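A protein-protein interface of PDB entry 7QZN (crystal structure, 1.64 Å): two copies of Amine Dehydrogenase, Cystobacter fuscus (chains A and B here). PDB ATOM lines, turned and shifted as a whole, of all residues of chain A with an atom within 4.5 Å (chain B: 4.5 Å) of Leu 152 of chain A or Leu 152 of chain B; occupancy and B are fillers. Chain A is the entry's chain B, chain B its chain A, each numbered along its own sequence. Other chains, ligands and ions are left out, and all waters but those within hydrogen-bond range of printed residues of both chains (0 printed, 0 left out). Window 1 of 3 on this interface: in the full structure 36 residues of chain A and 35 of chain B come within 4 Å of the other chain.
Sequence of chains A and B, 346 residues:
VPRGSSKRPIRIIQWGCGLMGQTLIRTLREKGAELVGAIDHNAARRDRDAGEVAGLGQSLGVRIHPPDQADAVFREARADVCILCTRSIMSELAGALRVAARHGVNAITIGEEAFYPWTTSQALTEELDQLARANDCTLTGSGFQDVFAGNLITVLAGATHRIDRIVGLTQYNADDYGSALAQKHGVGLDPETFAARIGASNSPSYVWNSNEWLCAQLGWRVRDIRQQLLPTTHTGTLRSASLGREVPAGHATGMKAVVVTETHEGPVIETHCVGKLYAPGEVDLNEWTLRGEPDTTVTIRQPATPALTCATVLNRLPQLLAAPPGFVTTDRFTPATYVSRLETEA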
ATOM      1  N   VAL A 147      22.914  27.728   5.369  1.00  0.00           N
ATOM      2  CA  VAL A 147      23.187  26.949   4.141  1.00  0.00           C
ATOM      3  C   VAL A 147      23.191  25.456   4.467  1.00  0.00           C
ATOM      4  O   VAL A 147      22.478  24.718   3.729  1.00  0.00           O
ATOM      5  CB  VAL A 147      24.514  27.403   3.521  1.00  0.00           C
ATOM      6  CG1 VAL A 147      24.930  26.479   2.406  1.00  0.00           C
ATOM      7  CG2 VAL A 147      24.358  28.824   3.018  1.00  0.00           C
ATOM      8  N   PHE A 148      23.966  25.009   5.464  1.00  0.00           N
ATOM      9  CA  PHE A 148      24.402  23.580   5.537  1.00  0.00           C
ATOM     10  C   PHE A 148      23.366  22.682   6.215  1.00  0.00           C
ATOM     11  O   PHE A 148      23.572  21.449   6.241  1.00  0.00           O
ATOM     12  CB  PHE A 148      25.806  23.540   6.150  1.00  0.00           C
ATOM     13  CG  PHE A 148      26.797  24.159   5.211  1.00  0.00           C
ATOM     14  CD1 PHE A 148      27.355  23.451   4.167  1.00  0.00           C
ATOM     15  CD2 PHE A 148      27.195  25.468   5.391  1.00  0.00           C
ATOM     16  CE1 PHE A 148      28.247  24.043   3.290  1.00  0.00           C
ATOM     17  CE2 PHE A 148      28.044  26.071   4.486  1.00  0.00           C
ATOM     18  CZ  PHE A 148      28.606  25.349   3.466  1.00  0.00           C
ATOM     19  N   GLY A 150      19.951  23.872   5.435  1.00  0.00           N
ATOM     20  CA  GLY A 150      18.980  24.889   4.997  1.00  0.00           C
ATOM     21  C   GLY A 150      18.988  24.988   3.487  1.00  0.00           C
ATOM     22  O   GLY A 150      18.539  24.068   2.785  1.00  0.00           O
ATOM     23  N   ASN A 151      19.480  26.109   2.986  1.00  0.00           N
ATOM     24  CA  ASN A 151      19.434  26.380   1.536  1.00  0.00           C
ATOM     25  C   ASN A 151      20.275  25.416   0.672  1.00  0.00           C
ATOM     26  O   ASN A 151      19.937  25.301  -0.502  1.00  0.00           O
ATOM     27  CB  ASN A 151      19.809  27.832   1.234  1.00  0.00           C
ATOM     28  CG  ASN A 151      18.652  28.762   1.497  1.00  0.00           C
ATOM     29  OD1 ASN A 151      17.521  28.501   1.146  1.00  0.00           O
ATOM     30  ND2 ASN A 151      18.914  29.792   2.226  1.00  0.00           N
ATOM     31  N   LEU A 152      21.290  24.751   1.180  1.00  0.00           N
ATOM     32  CA  LEU A 152      21.919  23.665   0.382  1.00  0.00           C
ATOM     33  C   LEU A 152      20.876  22.608   0.030  1.00  0.00           C
ATOM     34  O   LEU A 152      20.827  22.164  -1.118  1.00  0.00           O
ATOM     35  CB  LEU A 152      23.050  23.030   1.163  1.00  0.00           C
ATOM     36  CG  LEU A 152      23.729  21.823   0.534  1.00  0.00           C
ATOM     37  CD1 LEU A 152      24.394  22.162  -0.760  1.00  0.00           C
ATOM     38  CD2 LEU A 152      24.745  21.288   1.514  1.00  0.00           C
ATOM     39  N   ILE A 153      20.028  22.273   0.992  1.00  0.00           N
ATOM     40  CA  ILE A 153      19.000  21.225   0.777  1.00  0.00           C
ATOM     41  C   ILE A 153      17.894  21.771  -0.156  1.00  0.00           C
ATOM     42  O   ILE A 153      17.459  21.053  -1.107  1.00  0.00           O
ATOM     43  CB  ILE A 153      18.421  20.727   2.121  1.00  0.00           C
ATOM     44  CG1 ILE A 153      19.442  19.960   2.965  1.00  0.00           C
ATOM     45  CG2 ILE A 153      17.201  19.862   1.852  1.00  0.00           C
ATOM     46  CD1 ILE A 153      20.621  20.755   3.473  1.00  0.00           C
ATOM     47  N   THR A 154      17.421  22.995   0.059  1.00  0.00           N
ATOM     48  CA  THR A 154      16.283  23.523  -0.722  1.00  0.00           C
ATOM     49  C   THR A 154      16.704  23.861  -2.163  1.00  0.00           C
ATOM     50  O   THR A 154      15.887  23.696  -3.065  1.00  0.00           O
ATOM     51  CB  THR A 154      15.605  24.688  -0.018  1.00  0.00           C
ATOM     52  OG1 THR A 154      16.534  25.757   0.107  1.00  0.00           O
ATOM     53  CG2 THR A 154      15.121  24.288   1.364  1.00  0.00           C
ATOM     54  N   VAL A 155      17.975  24.212  -2.372  1.00  0.00           N
ATOM     55  CA  VAL A 155      18.472  24.414  -3.749  1.00  0.00           C
ATOM     56  C   VAL A 155      18.440  23.068  -4.492  1.00  0.00           C
ATOM     57  O   VAL A 155      17.969  23.032  -5.635  1.00  0.00           O
ATOM     58  CB  VAL A 155      19.850  25.095  -3.773  1.00  0.00           C
ATOM     59  CG1 VAL A 155      20.981  24.192  -3.346  1.00  0.00           C
ATOM     60  CG2 VAL A 155      20.159  25.625  -5.156  1.00  0.00           C
ATOM     61  N   LEU A 156      18.852  21.973  -3.832  1.00  0.00           N
ATOM     62  CA  LEU A 156      18.811  20.642  -4.457  1.00  0.00           C
ATOM     63  C   LEU A 156      17.368  20.148  -4.622  1.00  0.00           C
ATOM     64  O   LEU A 156      17.094  19.516  -5.649  1.00  0.00           O
ATOM     65  CB  LEU A 156      19.685  19.672  -3.672  1.00  0.00           C
ATOM     66  CG  LEU A 156      21.164  20.044  -3.655  1.00  0.00           C
ATOM     67  CD1 LEU A 156      21.921  19.268  -2.581  1.00  0.00           C
ATOM     68  CD2 LEU A 156      21.771  19.784  -5.003  1.00  0.00           C
ATOM     69  N   ASN A 286      29.232  16.607   6.695  1.00  0.00           N
ATOM     70  CA  ASN A 286      27.945  17.167   6.217  1.00  0.00           C
ATOM     71  C   ASN A 286      27.559  16.374   4.985  1.00  0.00           C
ATOM     72  O   ASN A 286      28.275  16.416   3.969  1.00  0.00           O
ATOM     73  CB  ASN A 286      28.027  18.668   5.996  1.00  0.00           C
ATOM     74  CG  ASN A 286      26.666  19.317   5.828  1.00  0.00           C
ATOM     75  OD1 ASN A 286      26.126  19.925   6.766  1.00  0.00           O
ATOM     76  ND2 ASN A 286      26.105  19.141   4.662  1.00  0.00           N
ATOM     77  N   VAL A 298      24.509  14.682  -1.608  1.00  0.00           N
ATOM     78  CA  VAL A 298      25.509  15.778  -1.566  1.00  0.00           C
ATOM     79  C   VAL A 298      26.399  15.594  -0.346  1.00  0.00           C
ATOM     80  O   VAL A 298      25.907  15.294   0.765  1.00  0.00           O
ATOM     81  CB  VAL A 298      24.860  17.171  -1.587  1.00  0.00           C
ATOM     82  CG1 VAL A 298      23.917  17.366  -0.419  1.00  0.00           C
ATOM     83  CG2 VAL A 298      25.910  18.244  -1.645  1.00  0.00           C
ATOM     84  N   ILE A 300      29.644  17.607   1.691  1.00  0.00           N
ATOM     85  CA  ILE A 300      30.660  18.669   1.890  1.00  0.00           C
ATOM     86  C   ILE A 300      31.897  17.988   2.499  1.00  0.00           C
ATOM     87  O   ILE A 300      31.781  17.351   3.551  1.00  0.00           O
ATOM     88  CB  ILE A 300      30.135  19.860   2.716  1.00  0.00           C
ATOM     89  CG1 ILE A 300      28.801  20.385   2.198  1.00  0.00           C
ATOM     90  CG2 ILE A 300      31.180  20.949   2.793  1.00  0.00           C
ATOM     91  CD1 ILE A 300      28.853  20.885   0.767  1.00  0.00           C
ATOM     92  N   VAL B 147      20.949  24.532 -11.251  1.00  0.00           N
ATOM     93  CA  VAL B 147      21.498  24.245  -9.905  1.00  0.00           C
ATOM     94  C   VAL B 147      22.989  23.857 -10.021  1.00  0.00           C
ATOM     95  O   VAL B 147      23.810  24.453  -9.281  1.00  0.00           O
ATOM     96  CB  VAL B 147      20.678  23.149  -9.217  1.00  0.00           C
ATOM     97  CG1 VAL B 147      21.348  22.673  -7.945  1.00  0.00           C
ATOM     98  CG2 VAL B 147      19.291  23.677  -8.930  1.00  0.00           C
ATOM     99  N   PHE B 148      23.318  22.895 -10.869  1.00  0.00           N
ATOM    100  CA  PHE B 148      24.573  22.110 -10.770  1.00  0.00           C
ATOM    101  C   PHE B 148      25.780  22.818 -11.394  1.00  0.00           C
ATOM    102  O   PHE B 148      26.886  22.312 -11.234  1.00  0.00           O
ATOM    103  CB  PHE B 148      24.320  20.677 -11.237  1.00  0.00           C
ATOM    104  CG  PHE B 148      23.375  19.974 -10.300  1.00  0.00           C
ATOM    105  CD1 PHE B 148      23.804  19.458  -9.089  1.00  0.00           C
ATOM    106  CD2 PHE B 148      22.023  19.927 -10.594  1.00  0.00           C
ATOM    107  CE1 PHE B 148      22.915  18.833  -8.239  1.00  0.00           C
ATOM    108  CE2 PHE B 148      21.126  19.328  -9.720  1.00  0.00           C
ATOM    109  CZ  PHE B 148      21.578  18.766  -8.538  1.00  0.00           C
ATOM    110  N   GLY B 150      25.388  26.513 -11.139  1.00  0.00           N
ATOM    111  CA  GLY B 150      24.692  27.773 -10.853  1.00  0.00           C
ATOM    112  C   GLY B 150      24.376  27.931  -9.394  1.00  0.00           C
ATOM    113  O   GLY B 150      25.275  28.274  -8.638  1.00  0.00           O
ATOM    114  N   ASN B 151      23.105  27.786  -9.011  1.00  0.00           N
ATOM    115  CA  ASN B 151      22.702  28.078  -7.618  1.00  0.00           C
ATOM    116  C   ASN B 151      23.358  27.184  -6.571  1.00  0.00           C
ATOM    117  O   ASN B 151      23.519  27.653  -5.434  1.00  0.00           O
ATOM    118  CB  ASN B 151      21.193  28.111  -7.454  1.00  0.00           C
ATOM    119  CG  ASN B 151      20.599  29.416  -7.948  1.00  0.00           C
ATOM    120  OD1 ASN B 151      21.044  30.505  -7.597  1.00  0.00           O
ATOM    121  ND2 ASN B 151      19.651  29.309  -8.844  1.00  0.00           N
ATOM    122  N   LEU B 152      23.800  25.967  -6.899  1.00  0.00           N
ATOM    123  CA  LEU B 152      24.576  25.214  -5.894  1.00  0.00           C
ATOM    124  C   LEU B 152      25.820  26.009  -5.497  1.00  0.00           C
ATOM    125  O   LEU B 152      26.163  26.074  -4.313  1.00  0.00           O
ATOM    126  CB  LEU B 152      24.965  23.855  -6.451  1.00  0.00           C
ATOM    127  CG  LEU B 152      25.864  22.992  -5.578  1.00  0.00           C
ATOM    128  CD1 LEU B 152      25.165  22.639  -4.284  1.00  0.00           C
ATOM    129  CD2 LEU B 152      26.191  21.705  -6.311  1.00  0.00           C
ATOM    130  N   ILE B 153      26.493  26.582  -6.472  1.00  0.00           N
ATOM    131  CA  ILE B 153      27.744  27.367  -6.238  1.00  0.00           C
ATOM    132  C   ILE B 153      27.422  28.671  -5.510  1.00  0.00           C
ATOM    133  O   ILE B 153      28.137  29.022  -4.515  1.00  0.00           O
ATOM    134  CB  ILE B 153      28.474  27.607  -7.565  1.00  0.00           C
ATOM    135  CG1 ILE B 153      29.007  26.283  -8.129  1.00  0.00           C
ATOM    136  CG2 ILE B 153      29.606  28.595  -7.346  1.00  0.00           C
ATOM    137  CD1 ILE B 153      27.991  25.352  -8.706  1.00  0.00           C
ATOM    138  N   THR B 154      26.386  29.383  -5.900  1.00  0.00           N
ATOM    139  CA  THR B 154      26.116  30.723  -5.325  1.00  0.00           C
ATOM    140  C   THR B 154      25.541  30.554  -3.908  1.00  0.00           C
ATOM    141  O   THR B 154      25.784  31.433  -3.056  1.00  0.00           O
ATOM    142  CB  THR B 154      25.241  31.562  -6.241  1.00  0.00           C
ATOM    143  OG1 THR B 154      23.980  30.916  -6.416  1.00  0.00           O
ATOM    144  CG2 THR B 154      25.921  31.797  -7.567  1.00  0.00           C
ATOM    145  N   VAL B 155      24.792  29.480  -3.648  1.00  0.00           N
ATOM    146  CA  VAL B 155      24.330  29.186  -2.261  1.00  0.00           C
ATOM    147  C   VAL B 155      25.557  28.958  -1.362  1.00  0.00           C
ATOM    148  O   VAL B 155      25.604  29.543  -0.284  1.00  0.00           O
ATOM    149  CB  VAL B 155      23.300  28.045  -2.187  1.00  0.00           C
ATOM    150  CG1 VAL B 155      23.042  27.639  -0.751  1.00  0.00           C
ATOM    151  CG2 VAL B 155      21.982  28.457  -2.790  1.00  0.00           C
ATOM    152  N   LEU B 156      26.566  28.211  -1.819  1.00  0.00           N
ATOM    153  CA  LEU B 156      27.790  28.022  -1.029  1.00  0.00           C
ATOM    154  C   LEU B 156      28.598  29.320  -0.918  1.00  0.00           C
ATOM    155  O   LEU B 156      29.178  29.562   0.172  1.00  0.00           O
ATOM    156  CB  LEU B 156      28.592  26.862  -1.620  1.00  0.00           C
ATOM    157  CG  LEU B 156      27.881  25.516  -1.538  1.00  0.00           C
ATOM    158  CD1 LEU B 156      28.535  24.489  -2.437  1.00  0.00           C
ATOM    159  CD2 LEU B 156      27.822  25.010  -0.096  1.00  0.00           C
ATOM    160  N   ASN B 286      30.143  15.625 -10.454  1.00  0.00           N
ATOM    161  CA  ASN B 286      29.870  17.057 -10.179  1.00  0.00           C
ATOM    162  C   ASN B 286      30.580  17.396  -8.901  1.00  0.00           C
ATOM    163  O   ASN B 286      30.220  16.854  -7.847  1.00  0.00           O
ATOM    164  CB  ASN B 286      28.380  17.353 -10.148  1.00  0.00           C
ATOM    165  CG  ASN B 286      28.080  18.838 -10.234  1.00  0.00           C
ATOM    166  OD1 ASN B 286      27.789  19.375 -11.315  1.00  0.00           O
ATOM    167  ND2 ASN B 286      28.264  19.499  -9.122  1.00  0.00           N
ATOM    168  N   VAL B 298      32.249  20.773  -2.440  1.00  0.00           N
ATOM    169  CA  VAL B 298      30.949  20.060  -2.562  1.00  0.00           C
ATOM    170  C   VAL B 298      31.061  19.004  -3.658  1.00  0.00           C
ATOM    171  O   VAL B 298      31.571  19.272  -4.767  1.00  0.00           O
ATOM    172  CB  VAL B 298      29.782  21.005  -2.828  1.00  0.00           C
ATOM    173  CG1 VAL B 298      29.953  21.812  -4.121  1.00  0.00           C
ATOM    174  CG2 VAL B 298      28.468  20.253  -2.829  1.00  0.00           C
ATOM    175  N   ILE B 300      28.514  16.113  -5.606  1.00  0.00           N
ATOM    176  CA  ILE B 300      27.269  15.323  -5.839  1.00  0.00           C
ATOM    177  C   ILE B 300      27.715  13.912  -6.223  1.00  0.00           C
ATOM    178  O   ILE B 300      28.457  13.759  -7.182  1.00  0.00           O
ATOM    179  CB  ILE B 300      26.345  15.974  -6.890  1.00  0.00           C
ATOM    180  CG1 ILE B 300      26.129  17.474  -6.636  1.00  0.00           C
ATOM    181  CG2 ILE B 300      25.042  15.201  -6.978  1.00  0.00           C
ATOM    182  CD1 ILE B 300      25.465  17.730  -5.314  1.00  0.00           C
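Of the 12 printed residues of chain B, 8 touch a printed residue of chain A.
Hydrophobic or aromatic side chains of chain B within 4 Å of the printed part of chain A: Val 147, Phe 148, Leu 152, Val 155, Leu 156, Val 298 and Ile 300.
Of the 12 printed residues of chain A, 8 touch a printed residue of chain B.
Printed residues of chain A that touch a printed residue of chain B: Val 147, Phe 148, Asn 151, Leu 152, Val 155, Leu 156, Val 298 and Ile 300.
Among the printed residues, no Asp or Glu carboxylate lies within 4 Å of a Lys or Arg side-chain nitrogen of the other chain.
Val 147 of chain A touches Val 155 of chain B (CG2 to O, 3.6 Å).
CD2 of Leu 156 of chain B touches CE1 of Phe 148 of chain A, at 3.5 Å.
Asn 151 of chain A touches Val 155 of chain B (CB to CG1, 3.8 Å).
CD1 of Leu 152 of chain B touches CD1 of Leu 152 of chain A (3.6 Å).
Leu 152 of chain A touches Val 155 of chain B (N to CG1, 3.9 Å).
O of Val 155 of chain A touches CG2 of Val 147 of chain B (3.6 Å).
CB of Asn 151 of chain B touches CG2 of Val 155 of chain A, at 3.5 Å.
Leu 156 of chain A touches Phe 148 of chain B.
Ile 300 of chain B touches Val 298 of chain A (CD1 to CG2, 3.7 Å).
CG2 of Val 298 of chain B touches CD1 of Ile 300 of chain A (3.7 Å).
Val 147 of chain A touches Val 155 of chain B, and with the chains exchanged Val 155 of chain A touches Val 147 of chain B.
Leu 152 of chain A touches its own counterpart, Leu 152 of chain B.
Leu 152 of chain A touches Val 155 of chain B, but with the chains exchanged Val 155 of chain A does not touch Leu 152 of chain B (4.1 Å).
Val 298 of chain B touches its own counterpart, Val 298 of chain A.
Printed residues of chain B within 4 Å of Asn 151 of chain A: Val 155 (3.8 Å).
Leu 152 of chain A touches just these residues of chain B: Leu 152 and Val 155.
Printed residues of chain B within 4 Å of Val 155 of chain A: Val 147 (3.6 Å) and Asn 151 (3.5 Å).
Printed residues of chain B within 4 Å of Ile 300 of chain A: Val 298 (3.7 Å).
Of chain A, only Leu 152 (3.6 Å) comes within 4 Å of Leu 152 of chain B.
Ile 153 of chain B touches none of the printed residues of chain A.
Of the printed residues of chain A, Val 155 of chain B touches Val 147, Asn 151 and Leu 152.
Of the printed residues of chain A, Leu 156 of chain B touches Phe 148.
Asn 286 of chain B touches none of the printed residues of chain A.
The nearest printed residue of chain B that does not touch Leu 152 of chain A is Leu 156 of chain B (4.5 Å).
The nearest residue of chain A that does not touch Leu 152 of chain B is Val 155 of chain A (4.1 Å).
The backbone NH (N) of Leu 152 of chain A sits at hydrogen-bond distance from the backbone carbonyl oxygen (O) of Val 147 of chain A.
The backbone carbonyl oxygen (O) of Phe 148 of chain B sits close to the side-chain amide oxygen (OD1) of Asn 286 of chain B (3.1 Å).
The backbone carbonyl oxygen (O) of Asn 286 of chain A lies within hydrogen-bond range of the backbone NH (N) of Ile 300 of chain A, at 2.9 Å.
OD1 of Asn 151 of chain B is in hydrogen-bond range of OG1 of Thr 154 of chain B, at 3.2 Å.
The backbone NH (N) of Leu 152 of chain B sits at hydrogen-bond distance from the backbone carbonyl oxygen (O) of Val 147 of chain B, at 2.8 Å.
N of Ile 300 of chain B lies within hydrogen-bond range of O of Asn 286 of chain B (2.9 Å).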
